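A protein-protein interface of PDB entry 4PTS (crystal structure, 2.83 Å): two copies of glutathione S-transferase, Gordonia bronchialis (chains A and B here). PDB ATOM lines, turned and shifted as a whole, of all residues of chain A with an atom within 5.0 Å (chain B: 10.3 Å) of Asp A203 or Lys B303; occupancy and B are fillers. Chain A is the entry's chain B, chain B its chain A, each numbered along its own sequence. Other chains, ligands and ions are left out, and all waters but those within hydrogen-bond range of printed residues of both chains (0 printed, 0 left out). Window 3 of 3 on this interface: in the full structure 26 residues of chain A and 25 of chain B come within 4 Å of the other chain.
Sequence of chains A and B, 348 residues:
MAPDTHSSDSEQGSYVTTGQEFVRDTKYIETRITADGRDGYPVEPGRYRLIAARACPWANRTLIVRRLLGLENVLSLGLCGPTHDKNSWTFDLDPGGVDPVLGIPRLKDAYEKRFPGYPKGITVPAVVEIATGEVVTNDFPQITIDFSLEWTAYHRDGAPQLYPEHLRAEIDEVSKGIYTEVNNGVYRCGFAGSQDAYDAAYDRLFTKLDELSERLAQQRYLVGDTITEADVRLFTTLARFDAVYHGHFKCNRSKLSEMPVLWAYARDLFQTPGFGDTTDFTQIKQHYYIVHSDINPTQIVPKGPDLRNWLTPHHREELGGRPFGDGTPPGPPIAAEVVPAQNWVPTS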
ATOM      1  N   TYR A 198     -11.122  21.191  15.891  1.00  0.00           N
ATOM      2  CA  TYR A 198     -11.425  19.774  15.929  1.00  0.00           C
ATOM      3  C   TYR A 198     -11.435  19.201  17.352  1.00  0.00           C
ATOM      4  O   TYR A 198     -12.373  18.488  17.745  1.00  0.00           O
ATOM      5  CB  TYR A 198     -10.419  19.009  15.091  1.00  0.00           C
ATOM      6  CG  TYR A 198     -10.469  17.553  15.381  1.00  0.00           C
ATOM      7  CD1 TYR A 198     -11.470  16.752  14.845  1.00  0.00           C
ATOM      8  CD2 TYR A 198      -9.547  16.963  16.210  1.00  0.00           C
ATOM      9  CE1 TYR A 198     -11.536  15.399  15.109  1.00  0.00           C
ATOM     10  CE2 TYR A 198      -9.603  15.601  16.481  1.00  0.00           C
ATOM     11  CZ  TYR A 198     -10.602  14.826  15.928  1.00  0.00           C
ATOM     12  OH  TYR A 198     -10.659  13.485  16.204  1.00  0.00           O
ATOM     13  N   ASP A 199     -10.394  19.531  18.118  1.00  0.00           N
ATOM     14  CA  ASP A 199     -10.238  19.029  19.484  1.00  0.00           C
ATOM     15  C   ASP A 199     -11.442  19.351  20.356  1.00  0.00           C
ATOM     16  O   ASP A 199     -11.915  18.515  21.148  1.00  0.00           O
ATOM     17  CB  ASP A 199      -8.994  19.624  20.136  1.00  0.00           C
ATOM     18  CG  ASP A 199      -7.688  19.063  19.558  1.00  0.00           C
ATOM     19  OD1 ASP A 199      -7.607  17.840  19.295  1.00  0.00           O
ATOM     20  OD2 ASP A 199      -6.724  19.845  19.377  1.00  0.00           O
ATOM     21  N   ALA A 200     -11.943  20.565  20.173  1.00  0.00           N
ATOM     22  CA  ALA A 200     -13.066  21.064  20.943  1.00  0.00           C
ATOM     23  C   ALA A 200     -14.332  20.315  20.586  1.00  0.00           C
ATOM     24  O   ALA A 200     -15.094  19.914  21.470  1.00  0.00           O
ATOM     25  CB  ALA A 200     -13.252  22.545  20.673  1.00  0.00           C
ATOM     26  N   ALA A 201     -14.561  20.139  19.291  1.00  0.00           N
ATOM     27  CA  ALA A 201     -15.713  19.404  18.845  1.00  0.00           C
ATOM     28  C   ALA A 201     -15.694  17.974  19.378  1.00  0.00           C
ATOM     29  O   ALA A 201     -16.714  17.464  19.827  1.00  0.00           O
ATOM     30  CB  ALA A 201     -15.781  19.399  17.331  1.00  0.00           C
ATOM     31  N   TYR A 202     -14.537  17.329  19.288  1.00  0.00           N
ATOM     32  CA  TYR A 202     -14.394  15.939  19.685  1.00  0.00           C
ATOM     33  C   TYR A 202     -14.836  15.791  21.137  1.00  0.00           C
ATOM     34  O   TYR A 202     -15.607  14.878  21.480  1.00  0.00           O
ATOM     35  CB  TYR A 202     -12.948  15.505  19.485  1.00  0.00           C
ATOM     36  CG  TYR A 202     -12.566  14.118  19.986  1.00  0.00           C
ATOM     37  CD1 TYR A 202     -12.305  13.892  21.324  1.00  0.00           C
ATOM     38  CD2 TYR A 202     -12.392  13.052  19.112  1.00  0.00           C
ATOM     39  CE1 TYR A 202     -11.917  12.635  21.791  1.00  0.00           C
ATOM     40  CE2 TYR A 202     -12.008  11.786  19.571  1.00  0.00           C
ATOM     41  CZ  TYR A 202     -11.764  11.595  20.914  1.00  0.00           C
ATOM     42  OH  TYR A 202     -11.387  10.388  21.413  1.00  0.00           O
ATOM     43  N   ASP A 203     -14.402  16.712  21.984  1.00  0.00           N
ATOM     44  CA  ASP A 203     -14.740  16.600  23.385  1.00  0.00           C
ATOM     45  C   ASP A 203     -16.248  16.750  23.619  1.00  0.00           C
ATOM     46  O   ASP A 203     -16.879  15.954  24.320  1.00  0.00           O
ATOM     47  CB  ASP A 203     -13.969  17.642  24.176  1.00  0.00           C
ATOM     48  CG  ASP A 203     -12.447  17.393  24.175  1.00  0.00           C
ATOM     49  OD1 ASP A 203     -12.015  16.207  24.159  1.00  0.00           O
ATOM     50  OD2 ASP A 203     -11.692  18.401  24.222  1.00  0.00           O
ATOM     51  N   ARG A 204     -16.842  17.757  23.009  1.00  0.00           N
ATOM     52  CA  ARG A 204     -18.253  17.994  23.205  1.00  0.00           C
ATOM     53  C   ARG A 204     -19.081  16.825  22.729  1.00  0.00           C
ATOM     54  O   ARG A 204     -20.051  16.430  23.375  1.00  0.00           O
ATOM     55  CB  ARG A 204     -18.654  19.296  22.524  1.00  0.00           C
ATOM     56  CG  ARG A 204     -18.233  20.491  23.371  1.00  0.00           C
ATOM     57  CD  ARG A 204     -18.574  21.800  22.710  1.00  0.00           C
ATOM     58  NE  ARG A 204     -20.006  21.944  22.478  1.00  0.00           N
ATOM     59  CZ  ARG A 204     -20.547  22.849  21.668  1.00  0.00           C
ATOM     60  NH1 ARG A 204     -19.781  23.719  21.024  1.00  0.00           N
ATOM     61  NH2 ARG A 204     -21.867  22.893  21.494  1.00  0.00           N
ATOM     62  N   LEU A 205     -18.673  16.261  21.610  1.00  0.00           N
ATOM     63  CA  LEU A 205     -19.331  15.113  21.036  1.00  0.00           C
ATOM     64  C   LEU A 205     -19.378  13.930  22.004  1.00  0.00           C
ATOM     65  O   LEU A 205     -20.425  13.329  22.239  1.00  0.00           O
ATOM     66  CB  LEU A 205     -18.568  14.702  19.800  1.00  0.00           C
ATOM     67  CG  LEU A 205     -19.074  13.490  19.030  1.00  0.00           C
ATOM     68  CD1 LEU A 205     -20.492  13.719  18.535  1.00  0.00           C
ATOM     69  CD2 LEU A 205     -18.148  13.225  17.856  1.00  0.00           C
ATOM     70  N   PHE A 206     -18.233  13.590  22.560  1.00  0.00           N
ATOM     71  CA  PHE A 206     -18.158  12.377  23.325  1.00  0.00           C
ATOM     72  C   PHE A 206     -18.658  12.550  24.757  1.00  0.00           C
ATOM     73  O   PHE A 206     -19.182  11.609  25.346  1.00  0.00           O
ATOM     74  CB  PHE A 206     -16.759  11.786  23.231  1.00  0.00           C
ATOM     75  CG  PHE A 206     -16.516  11.097  21.930  1.00  0.00           C
ATOM     76  CD1 PHE A 206     -17.043   9.846  21.696  1.00  0.00           C
ATOM     77  CD2 PHE A 206     -15.833  11.724  20.903  1.00  0.00           C
ATOM     78  CE1 PHE A 206     -16.868   9.219  20.480  1.00  0.00           C
ATOM     79  CE2 PHE A 206     -15.641  11.096  19.677  1.00  0.00           C
ATOM     80  CZ  PHE A 206     -16.169   9.846  19.467  1.00  0.00           C
ATOM     81  N   THR A 207     -18.566  13.757  25.290  1.00  0.00           N
ATOM     82  CA  THR A 207     -19.259  14.085  26.532  1.00  0.00           C
ATOM     83  C   THR A 207     -20.747  13.844  26.383  1.00  0.00           C
ATOM     84  O   THR A 207     -21.368  13.227  27.240  1.00  0.00           O
ATOM     85  CB  THR A 207     -19.084  15.570  26.876  1.00  0.00           C
ATOM     86  OG1 THR A 207     -17.697  15.830  27.076  1.00  0.00           O
ATOM     87  CG2 THR A 207     -19.842  15.940  28.141  1.00  0.00           C
ATOM     88  N   LYS A 208     -21.310  14.357  25.293  1.00  0.00           N
ATOM     89  CA  LYS A 208     -22.723  14.201  25.048  1.00  0.00           C
ATOM     90  C   LYS A 208     -23.106  12.743  24.924  1.00  0.00           C
ATOM     91  O   LYS A 208     -24.151  12.328  25.421  1.00  0.00           O
ATOM     92  CB  LYS A 208     -23.161  14.924  23.775  1.00  0.00           C
ATOM     93  CG  LYS A 208     -24.680  14.962  23.601  1.00  0.00           C
ATOM     94  CD  LYS A 208     -25.300  15.712  24.760  1.00  0.00           C
ATOM     95  CE  LYS A 208     -26.768  16.006  24.585  1.00  0.00           C
ATOM     96  NZ  LYS A 208     -27.151  16.922  25.695  1.00  0.00           N
ATOM     97  N   ASN A 252     -13.378   9.533  16.462  1.00  0.00           N
ATOM     98  CA  ASN A 252     -12.866   8.176  16.630  1.00  0.00           C
ATOM     99  C   ASN A 252     -12.417   7.726  18.013  1.00  0.00           C
ATOM    100  O   ASN A 252     -11.569   6.823  18.100  1.00  0.00           O
ATOM    101  CB  ASN A 252     -11.720   7.954  15.654  1.00  0.00           C
ATOM    102  CG  ASN A 252     -10.474   8.657  16.083  1.00  0.00           C
ATOM    103  OD1 ASN A 252     -10.518   9.632  16.802  1.00  0.00           O
ATOM    104  ND2 ASN A 252      -9.363   8.165  15.640  1.00  0.00           N
ATOM    105  N   ASP B 242      -5.584   0.239  14.732  1.00  0.00           N
ATOM    106  CA  ASP B 242      -6.672   1.140  15.166  1.00  0.00           C
ATOM    107  C   ASP B 242      -6.272   2.627  15.174  1.00  0.00           C
ATOM    108  O   ASP B 242      -7.056   3.501  14.813  1.00  0.00           O
ATOM    109  CB  ASP B 242      -7.198   0.727  16.532  1.00  0.00           C
ATOM    110  CG  ASP B 242      -8.097  -0.519  16.469  1.00  0.00           C
ATOM    111  OD1 ASP B 242      -8.314  -1.076  15.370  1.00  0.00           O
ATOM    112  OD2 ASP B 242      -8.603  -0.933  17.538  1.00  0.00           O
ATOM    113  N   ALA B 243      -5.029   2.914  15.521  1.00  0.00           N
ATOM    114  CA  ALA B 243      -4.593   4.285  15.579  1.00  0.00           C
ATOM    115  C   ALA B 243      -4.499   4.935  14.202  1.00  0.00           C
ATOM    116  O   ALA B 243      -4.738   6.133  14.069  1.00  0.00           O
ATOM    117  CB  ALA B 243      -3.266   4.372  16.306  1.00  0.00           C
ATOM    118  N   VAL B 244      -4.154   4.163  13.177  1.00  0.00           N
ATOM    119  CA  VAL B 244      -3.903   4.750  11.860  1.00  0.00           C
ATOM    120  C   VAL B 244      -4.553   4.021  10.699  1.00  0.00           C
ATOM    121  O   VAL B 244      -5.355   4.582   9.977  1.00  0.00           O
ATOM    122  CB  VAL B 244      -2.410   4.774  11.545  1.00  0.00           C
ATOM    123  CG1 VAL B 244      -2.180   5.537  10.252  1.00  0.00           C
ATOM    124  CG2 VAL B 244      -1.655   5.419  12.677  1.00  0.00           C
ATOM    125  N   PHE B 281       2.216   6.186  20.703  1.00  0.00           N
ATOM    126  CA  PHE B 281       1.032   6.422  19.905  1.00  0.00           C
ATOM    127  C   PHE B 281       0.899   7.872  19.440  1.00  0.00           C
ATOM    128  O   PHE B 281       0.292   8.147  18.413  1.00  0.00           O
ATOM    129  CB  PHE B 281      -0.191   6.061  20.698  1.00  0.00           C
ATOM    130  CG  PHE B 281      -0.269   4.621  21.063  1.00  0.00           C
ATOM    131  CD1 PHE B 281      -0.635   3.676  20.123  1.00  0.00           C
ATOM    132  CD2 PHE B 281      -0.005   4.198  22.359  1.00  0.00           C
ATOM    133  CE1 PHE B 281      -0.732   2.325  20.468  1.00  0.00           C
ATOM    134  CE2 PHE B 281      -0.107   2.858  22.710  1.00  0.00           C
ATOM    135  CZ  PHE B 281      -0.467   1.920  21.764  1.00  0.00           C
ATOM    136  N   THR B 282       1.440   8.817  20.181  1.00  0.00           N
ATOM    137  CA  THR B 282       1.288  10.169  19.734  1.00  0.00           C
ATOM    138  C   THR B 282       2.127  10.393  18.482  1.00  0.00           C
ATOM    139  O   THR B 282       1.630  10.932  17.499  1.00  0.00           O
ATOM    140  CB  THR B 282       1.595  11.190  20.840  1.00  0.00           C
ATOM    141  OG1 THR B 282       0.660  11.008  21.901  1.00  0.00           O
ATOM    142  CG2 THR B 282       1.465  12.649  20.322  1.00  0.00           C
ATOM    143  N   LYS B 285       0.600   8.579  15.258  1.00  0.00           N
ATOM    144  CA  LYS B 285      -0.476   9.316  14.640  1.00  0.00           C
ATOM    145  C   LYS B 285       0.030  10.594  13.994  1.00  0.00           C
ATOM    146  O   LYS B 285      -0.241  10.846  12.813  1.00  0.00           O
ATOM    147  CB  LYS B 285      -1.533   9.625  15.667  1.00  0.00           C
ATOM    148  CG  LYS B 285      -2.349   8.407  16.049  1.00  0.00           C
ATOM    149  CD  LYS B 285      -2.942   8.554  17.435  1.00  0.00           C
ATOM    150  CE  LYS B 285      -3.923   9.710  17.490  1.00  0.00           C
ATOM    151  NZ  LYS B 285      -4.473   9.914  18.855  1.00  0.00           N
ATOM    152  N   GLN B 286       0.807  11.371  14.736  1.00  0.00           N
ATOM    153  CA  GLN B 286       1.351  12.598  14.189  1.00  0.00           C
ATOM    154  C   GLN B 286       2.005  12.386  12.847  1.00  0.00           C
ATOM    155  O   GLN B 286       1.875  13.211  11.954  1.00  0.00           O
ATOM    156  CB  GLN B 286       2.378  13.191  15.124  1.00  0.00           C
ATOM    157  CG  GLN B 286       1.782  13.979  16.268  1.00  0.00           C
ATOM    158  CD  GLN B 286       2.815  14.411  17.287  1.00  0.00           C
ATOM    159  OE1 GLN B 286       3.924  13.871  17.353  1.00  0.00           O
ATOM    160  NE2 GLN B 286       2.454  15.387  18.101  1.00  0.00           N
ATOM    161  N   TYR B 289      -0.744  11.197   9.945  1.00  0.00           N
ATOM    162  CA  TYR B 289      -1.816  12.135   9.659  1.00  0.00           C
ATOM    163  C   TYR B 289      -1.270  13.482   9.215  1.00  0.00           C
ATOM    164  O   TYR B 289      -1.896  14.189   8.441  1.00  0.00           O
ATOM    165  CB  TYR B 289      -2.738  12.288  10.862  1.00  0.00           C
ATOM    166  CG  TYR B 289      -3.688  11.125  11.037  1.00  0.00           C
ATOM    167  CD1 TYR B 289      -4.855  11.039  10.285  1.00  0.00           C
ATOM    168  CD2 TYR B 289      -3.439  10.121  11.973  1.00  0.00           C
ATOM    169  CE1 TYR B 289      -5.739   9.980  10.448  1.00  0.00           C
ATOM    170  CE2 TYR B 289      -4.311   9.052  12.144  1.00  0.00           C
ATOM    171  CZ  TYR B 289      -5.464   8.971  11.378  1.00  0.00           C
ATOM    172  OH  TYR B 289      -6.345   7.893  11.533  1.00  0.00           O
ATOM    173  N   ASN B 296      -4.644  13.141   3.562  1.00  0.00           N
ATOM    174  CA  ASN B 296      -5.342  13.859   4.632  1.00  0.00           C
ATOM    175  C   ASN B 296      -4.914  15.306   4.667  1.00  0.00           C
ATOM    176  O   ASN B 296      -4.111  15.686   5.507  1.00  0.00           O
ATOM    177  CB  ASN B 296      -5.012  13.235   5.974  1.00  0.00           C
ATOM    178  CG  ASN B 296      -5.633  13.996   7.119  1.00  0.00           C
ATOM    179  OD1 ASN B 296      -6.775  14.445   7.018  1.00  0.00           O
ATOM    180  ND2 ASN B 296      -4.890  14.162   8.205  1.00  0.00           N
ATOM    181  N   GLN B 299      -4.540  17.754   7.661  1.00  0.00           N
ATOM    182  CA  GLN B 299      -3.419  17.442   8.587  1.00  0.00           C
ATOM    183  C   GLN B 299      -3.836  17.474  10.049  1.00  0.00           C
ATOM    184  O   GLN B 299      -3.032  17.708  10.946  1.00  0.00           O
ATOM    185  CB  GLN B 299      -2.219  18.358   8.363  1.00  0.00           C
ATOM    186  CG  GLN B 299      -1.794  18.411   6.916  1.00  0.00           C
ATOM    187  CD  GLN B 299      -0.540  19.212   6.724  1.00  0.00           C
ATOM    188  OE1 GLN B 299      -0.589  20.404   6.409  1.00  0.00           O
ATOM    189  NE2 GLN B 299       0.598  18.572   6.931  1.00  0.00           N
ATOM    190  N   ILE B 300      -5.115  17.229  10.265  1.00  0.00           N
ATOM    191  CA  ILE B 300      -5.632  17.140  11.580  1.00  0.00           C
ATOM    192  C   ILE B 300      -5.407  15.730  12.057  1.00  0.00           C
ATOM    193  O   ILE B 300      -5.660  14.777  11.342  1.00  0.00           O
ATOM    194  CB  ILE B 300      -7.113  17.508  11.594  1.00  0.00           C
ATOM    195  CG1 ILE B 300      -7.250  19.009  11.316  1.00  0.00           C
ATOM    196  CG2 ILE B 300      -7.745  17.185  12.946  1.00  0.00           C
ATOM    197  CD1 ILE B 300      -8.686  19.486  11.280  1.00  0.00           C
ATOM    198  N   VAL B 301      -4.943  15.611  13.285  1.00  0.00           N
ATOM    199  CA  VAL B 301      -4.722  14.329  13.894  1.00  0.00           C
ATOM    200  C   VAL B 301      -5.883  13.958  14.801  1.00  0.00           C
ATOM    201  O   VAL B 301      -6.204  14.679  15.724  1.00  0.00           O
ATOM    202  CB  VAL B 301      -3.461  14.360  14.761  1.00  0.00           C
ATOM    203  CG1 VAL B 301      -3.184  12.980  15.382  1.00  0.00           C
ATOM    204  CG2 VAL B 301      -2.289  14.865  13.943  1.00  0.00           C
ATOM    205  N   PRO B 302      -6.474  12.799  14.576  1.00  0.00           N
ATOM    206  CA  PRO B 302      -7.570  12.379  15.421  1.00  0.00           C
ATOM    207  C   PRO B 302      -7.132  12.264  16.843  1.00  0.00           C
ATOM    208  O   PRO B 302      -6.008  11.849  17.089  1.00  0.00           O
ATOM    209  CB  PRO B 302      -7.908  10.973  14.908  1.00  0.00           C
ATOM    210  CG  PRO B 302      -7.353  10.903  13.535  1.00  0.00           C
ATOM    211  CD  PRO B 302      -6.136  11.788  13.563  1.00  0.00           C
ATOM    212  N   LYS B 303      -8.006  12.636  17.770  1.00  0.00           N
ATOM    213  CA  LYS B 303      -7.711  12.487  19.189  1.00  0.00           C
ATOM    214  C   LYS B 303      -7.956  11.088  19.668  1.00  0.00           C
ATOM    215  O   LYS B 303      -7.404  10.700  20.667  1.00  0.00           O
ATOM    216  CB  LYS B 303      -8.494  13.476  20.034  1.00  0.00           C
ATOM    217  CG  LYS B 303      -7.742  14.784  20.184  1.00  0.00           C
ATOM    218  CD  LYS B 303      -8.444  15.711  21.147  1.00  0.00           C
ATOM    219  CE  LYS B 303      -8.442  15.184  22.574  1.00  0.00           C
ATOM    220  NZ  LYS B 303      -8.641  16.323  23.525  1.00  0.00           N
ATOM    221  N   GLY B 304      -8.779  10.332  18.947  1.00  0.00           N
ATOM    222  CA  GLY B 304      -8.992   8.920  19.252  1.00  0.00           C
ATOM    223  C   GLY B 304      -7.954   8.038  18.592  1.00  0.00           C
ATOM    224  O   GLY B 304      -7.034   8.531  17.950  1.00  0.00           O
ATOM    225  N   PRO B 305      -8.046   6.723  18.809  1.00  0.00           N
ATOM    226  CA  PRO B 305      -8.902   6.047  19.752  1.00  0.00           C
ATOM    227  C   PRO B 305      -8.417   6.134  21.182  1.00  0.00           C
ATOM    228  O   PRO B 305      -7.268   6.499  21.439  1.00  0.00           O
ATOM    229  CB  PRO B 305      -8.799   4.603  19.310  1.00  0.00           C
ATOM    230  CG  PRO B 305      -7.425   4.503  18.809  1.00  0.00           C
ATOM    231  CD  PRO B 305      -7.223   5.771  18.060  1.00  0.00           C
ATOM    232  N   ASP B 306      -9.307   5.771  22.095  1.00  0.00           N
ATOM    233  CA  ASP B 306      -8.963   5.604  23.485  1.00  0.00           C
ATOM    234  C   ASP B 306      -8.107   4.351  23.562  1.00  0.00           C
ATOM    235  O   ASP B 306      -8.507   3.288  23.086  1.00  0.00           O
ATOM    236  CB  ASP B 306     -10.225   5.442  24.357  1.00  0.00           C
ATOM    237  CG  ASP B 306      -9.903   4.981  25.788  1.00  0.00           C
ATOM    238  OD1 ASP B 306      -9.737   3.748  25.975  1.00  0.00           O
ATOM    239  OD2 ASP B 306      -9.798   5.832  26.711  1.00  0.00           O
ATOM    240  N   LEU B 307      -6.964   4.472  24.223  1.00  0.00           N
ATOM    241  CA  LEU B 307      -5.970   3.417  24.207  1.00  0.00           C
ATOM    242  C   LEU B 307      -6.053   2.468  25.375  1.00  0.00           C
ATOM    243  O   LEU B 307      -5.339   1.491  25.397  1.00  0.00           O
ATOM    244  CB  LEU B 307      -4.587   4.030  24.157  1.00  0.00           C
ATOM    245  CG  LEU B 307      -4.370   4.943  22.952  1.00  0.00           C
ATOM    246  CD1 LEU B 307      -3.106   5.754  23.149  1.00  0.00           C
ATOM    247  CD2 LEU B 307      -4.280   4.154  21.664  1.00  0.00           C
ATOM    248  N   ARG B 308      -6.951   2.717  26.312  1.00  0.00           N
ATOM    249  CA  ARG B 308      -6.904   2.024  27.593  1.00  0.00           C
ATOM    250  C   ARG B 308      -7.117   0.511  27.465  1.00  0.00           C
ATOM    251  O   ARG B 308      -6.527  -0.271  28.197  1.00  0.00           O
ATOM    252  CB  ARG B 308      -7.893   2.670  28.573  1.00  0.00           C
ATOM    253  CG  ARG B 308      -7.537   4.134  28.842  1.00  0.00           C
ATOM    254  CD  ARG B 308      -8.343   4.826  29.937  1.00  0.00           C
ATOM    255  NE  ARG B 308      -9.705   5.154  29.500  1.00  0.00           N
ATOM    256  CZ  ARG B 308     -10.462   6.136  29.998  1.00  0.00           C
ATOM    257  NH1 ARG B 308     -10.000   6.927  30.957  1.00  0.00           N
ATOM    258  NH2 ARG B 308     -11.695   6.328  29.532  1.00  0.00           N
ATOM    259  N   GLN B 342       2.232  10.833  28.790  1.00  0.00           N
ATOM    260  CA  GLN B 342       1.252  11.508  27.929  1.00  0.00           C
ATOM    261  C   GLN B 342       1.145  10.968  26.503  1.00  0.00           C
ATOM    262  O   GLN B 342       0.109  11.100  25.876  1.00  0.00           O
ATOM    263  CB  GLN B 342       1.642  12.970  27.825  1.00  0.00           C
ATOM    264  CG  GLN B 342       3.011  13.128  27.181  1.00  0.00           C
ATOM    265  CD  GLN B 342       3.724  14.407  27.558  1.00  0.00           C
ATOM    266  OE1 GLN B 342       4.847  14.365  28.067  1.00  0.00           O
ATOM    267  NE2 GLN B 342       3.073  15.556  27.315  1.00  0.00           N
ATOM    268  N   ASN B 343       2.227  10.394  25.988  1.00  0.00           N
ATOM    269  CA  ASN B 343       2.266   9.796  24.648  1.00  0.00           C
ATOM    270  C   ASN B 343       1.930   8.314  24.610  1.00  0.00           C
ATOM    271  O   ASN B 343       1.823   7.719  23.539  1.00  0.00           O
ATOM    272  CB  ASN B 343       3.666   9.956  24.060  1.00  0.00           C
ATOM    273  CG  ASN B 343       4.010  11.389  23.700  1.00  0.00           C
ATOM    274  OD1 ASN B 343       5.082  11.637  23.150  1.00  0.00           O
ATOM    275  ND2 ASN B 343       3.117  12.331  23.975  1.00  0.00           N
ATOM    276  N   TRP B 344       1.789   7.720  25.778  1.00  0.00           N
ATOM    277  CA  TRP B 344       1.525   6.299  25.897  1.00  0.00           C
ATOM    278  C   TRP B 344       0.071   6.121  26.269  1.00  0.00           C
ATOM    279  O   TRP B 344      -0.722   7.059  26.126  1.00  0.00           O
ATOM    280  CB  TRP B 344       2.434   5.717  26.978  1.00  0.00           C
ATOM    281  CG  TRP B 344       2.749   4.288  26.784  1.00  0.00           C
ATOM    282  CD1 TRP B 344       3.331   3.739  25.716  1.00  0.00           C
ATOM    283  CD2 TRP B 344       2.514   3.238  27.704  1.00  0.00           C
ATOM    284  NE1 TRP B 344       3.468   2.396  25.882  1.00  0.00           N
ATOM    285  CE2 TRP B 344       2.977   2.060  27.110  1.00  0.00           C
ATOM    286  CE3 TRP B 344       1.947   3.174  28.980  1.00  0.00           C
ATOM    287  CZ2 TRP B 344       2.892   0.812  27.743  1.00  0.00           C
ATOM    288  CZ3 TRP B 344       1.866   1.954  29.613  1.00  0.00           C
ATOM    289  CH2 TRP B 344       2.332   0.784  28.994  1.00  0.00           C
ATOM    290  N   PRO B 346      -2.917   6.052  28.907  1.00  0.00           N
ATOM    291  CA  PRO B 346      -3.198   6.671  30.235  1.00  0.00           C
ATOM    292  C   PRO B 346      -3.447   5.738  31.458  1.00  0.00           C
ATOM    293  O   PRO B 346      -4.066   4.668  31.342  1.00  0.00           O
ATOM    294  CB  PRO B 346      -4.464   7.482  29.972  1.00  0.00           C
ATOM    295  CG  PRO B 346      -4.395   7.805  28.518  1.00  0.00           C
ATOM    296  CD  PRO B 346      -3.849   6.565  27.879  1.00  0.00           C
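The side-chain carboxylate (OD1) of Asp A203 is in salt-bridge range of the side-chain amino group (NZ) of Lys B303 (3.4 Å). The side-chain amide oxygen of Asn A252 lies within hydrogen-bond range of the backbone NH of Gly B304, at 2.8 Å. The side-chain hydroxyl of Tyr A198 sits at hydrogen-bond distance from the backbone NH of Lys B303 (3.2 Å).
The backbone carbonyl oxygen (O) of Pro B302 sits close to the side-chain amino group (NZ) of Lys B285 (3.0 Å). The side-chain amino group of Lys B285 lies within hydrogen-bond range of the backbone carbonyl oxygen of Gly B304, at 3.0 Å. The backbone carbonyl oxygen (O) of Ile B300 lies within hydrogen-bond range of the side-chain amide nitrogen (ND2) of Asn B296 (3.3 Å). The backbone carbonyl oxygen of Asp A203 sits at hydrogen-bond distance from the side-chain hydroxyl of Thr A207, 2.9 Å away.
Among the printed residues, merely in contact across the chains: Asp A199 with Lys B303, Asn A252 with Pro B305, Asn A252 with Pro B302, Tyr A198 with Pro B302, Tyr A202 with Gly B304, Tyr A198 with Val B301, Tyr A198 with Ile B300 and Tyr A202 with Lys B303.
Asp A203 touches just one residue of chain B: Lys B303 (3.4 Å). No residue of chain B comes within 4 Å of Ala A201. Of chain B, only Lys B303 (3.9 Å) and Gly B304 (3.5 Å) come within 4 Å of Tyr A202. No residue of chain B comes within 4 Å of Thr A207. Printed residues of chain A within 4 Å of Pro B302: Tyr A198 (3.4 Å) and Asn A252 (3.2 Å). Of the printed residues of chain B, Tyr A198 touches Ile B300 (3.7 Å), Val B301 (3.6 Å), Pro B302 (3.4 Å) and Lys B303 (3.2 Å). Printed residues of chain A within 4 Å of Ile B300: Tyr A198 (3.7 Å). The nearest residue of chain B that does not touch Asp A203 is Gly B304 (8.5 Å). The nearest printed residue of chain A that does not touch Pro B302 is Tyr A202 (5.6 Å).
Hydrophobic or aromatic side chains of chain B that line the printed part of chain A: Ile B300, Pro B302 and Pro B305. Hydrophobic or aromatic side chains of chain A within 4 Å of the printed part of chain B: Tyr A198 and Tyr A202. Along chain A the printed residues that touch a printed residue of chain B span positions 198 to 252.
No position is printed for both chains. Of the 11 pairs that touch across the chains among the printed residues, none has its exchanged pair printed and touching as well.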
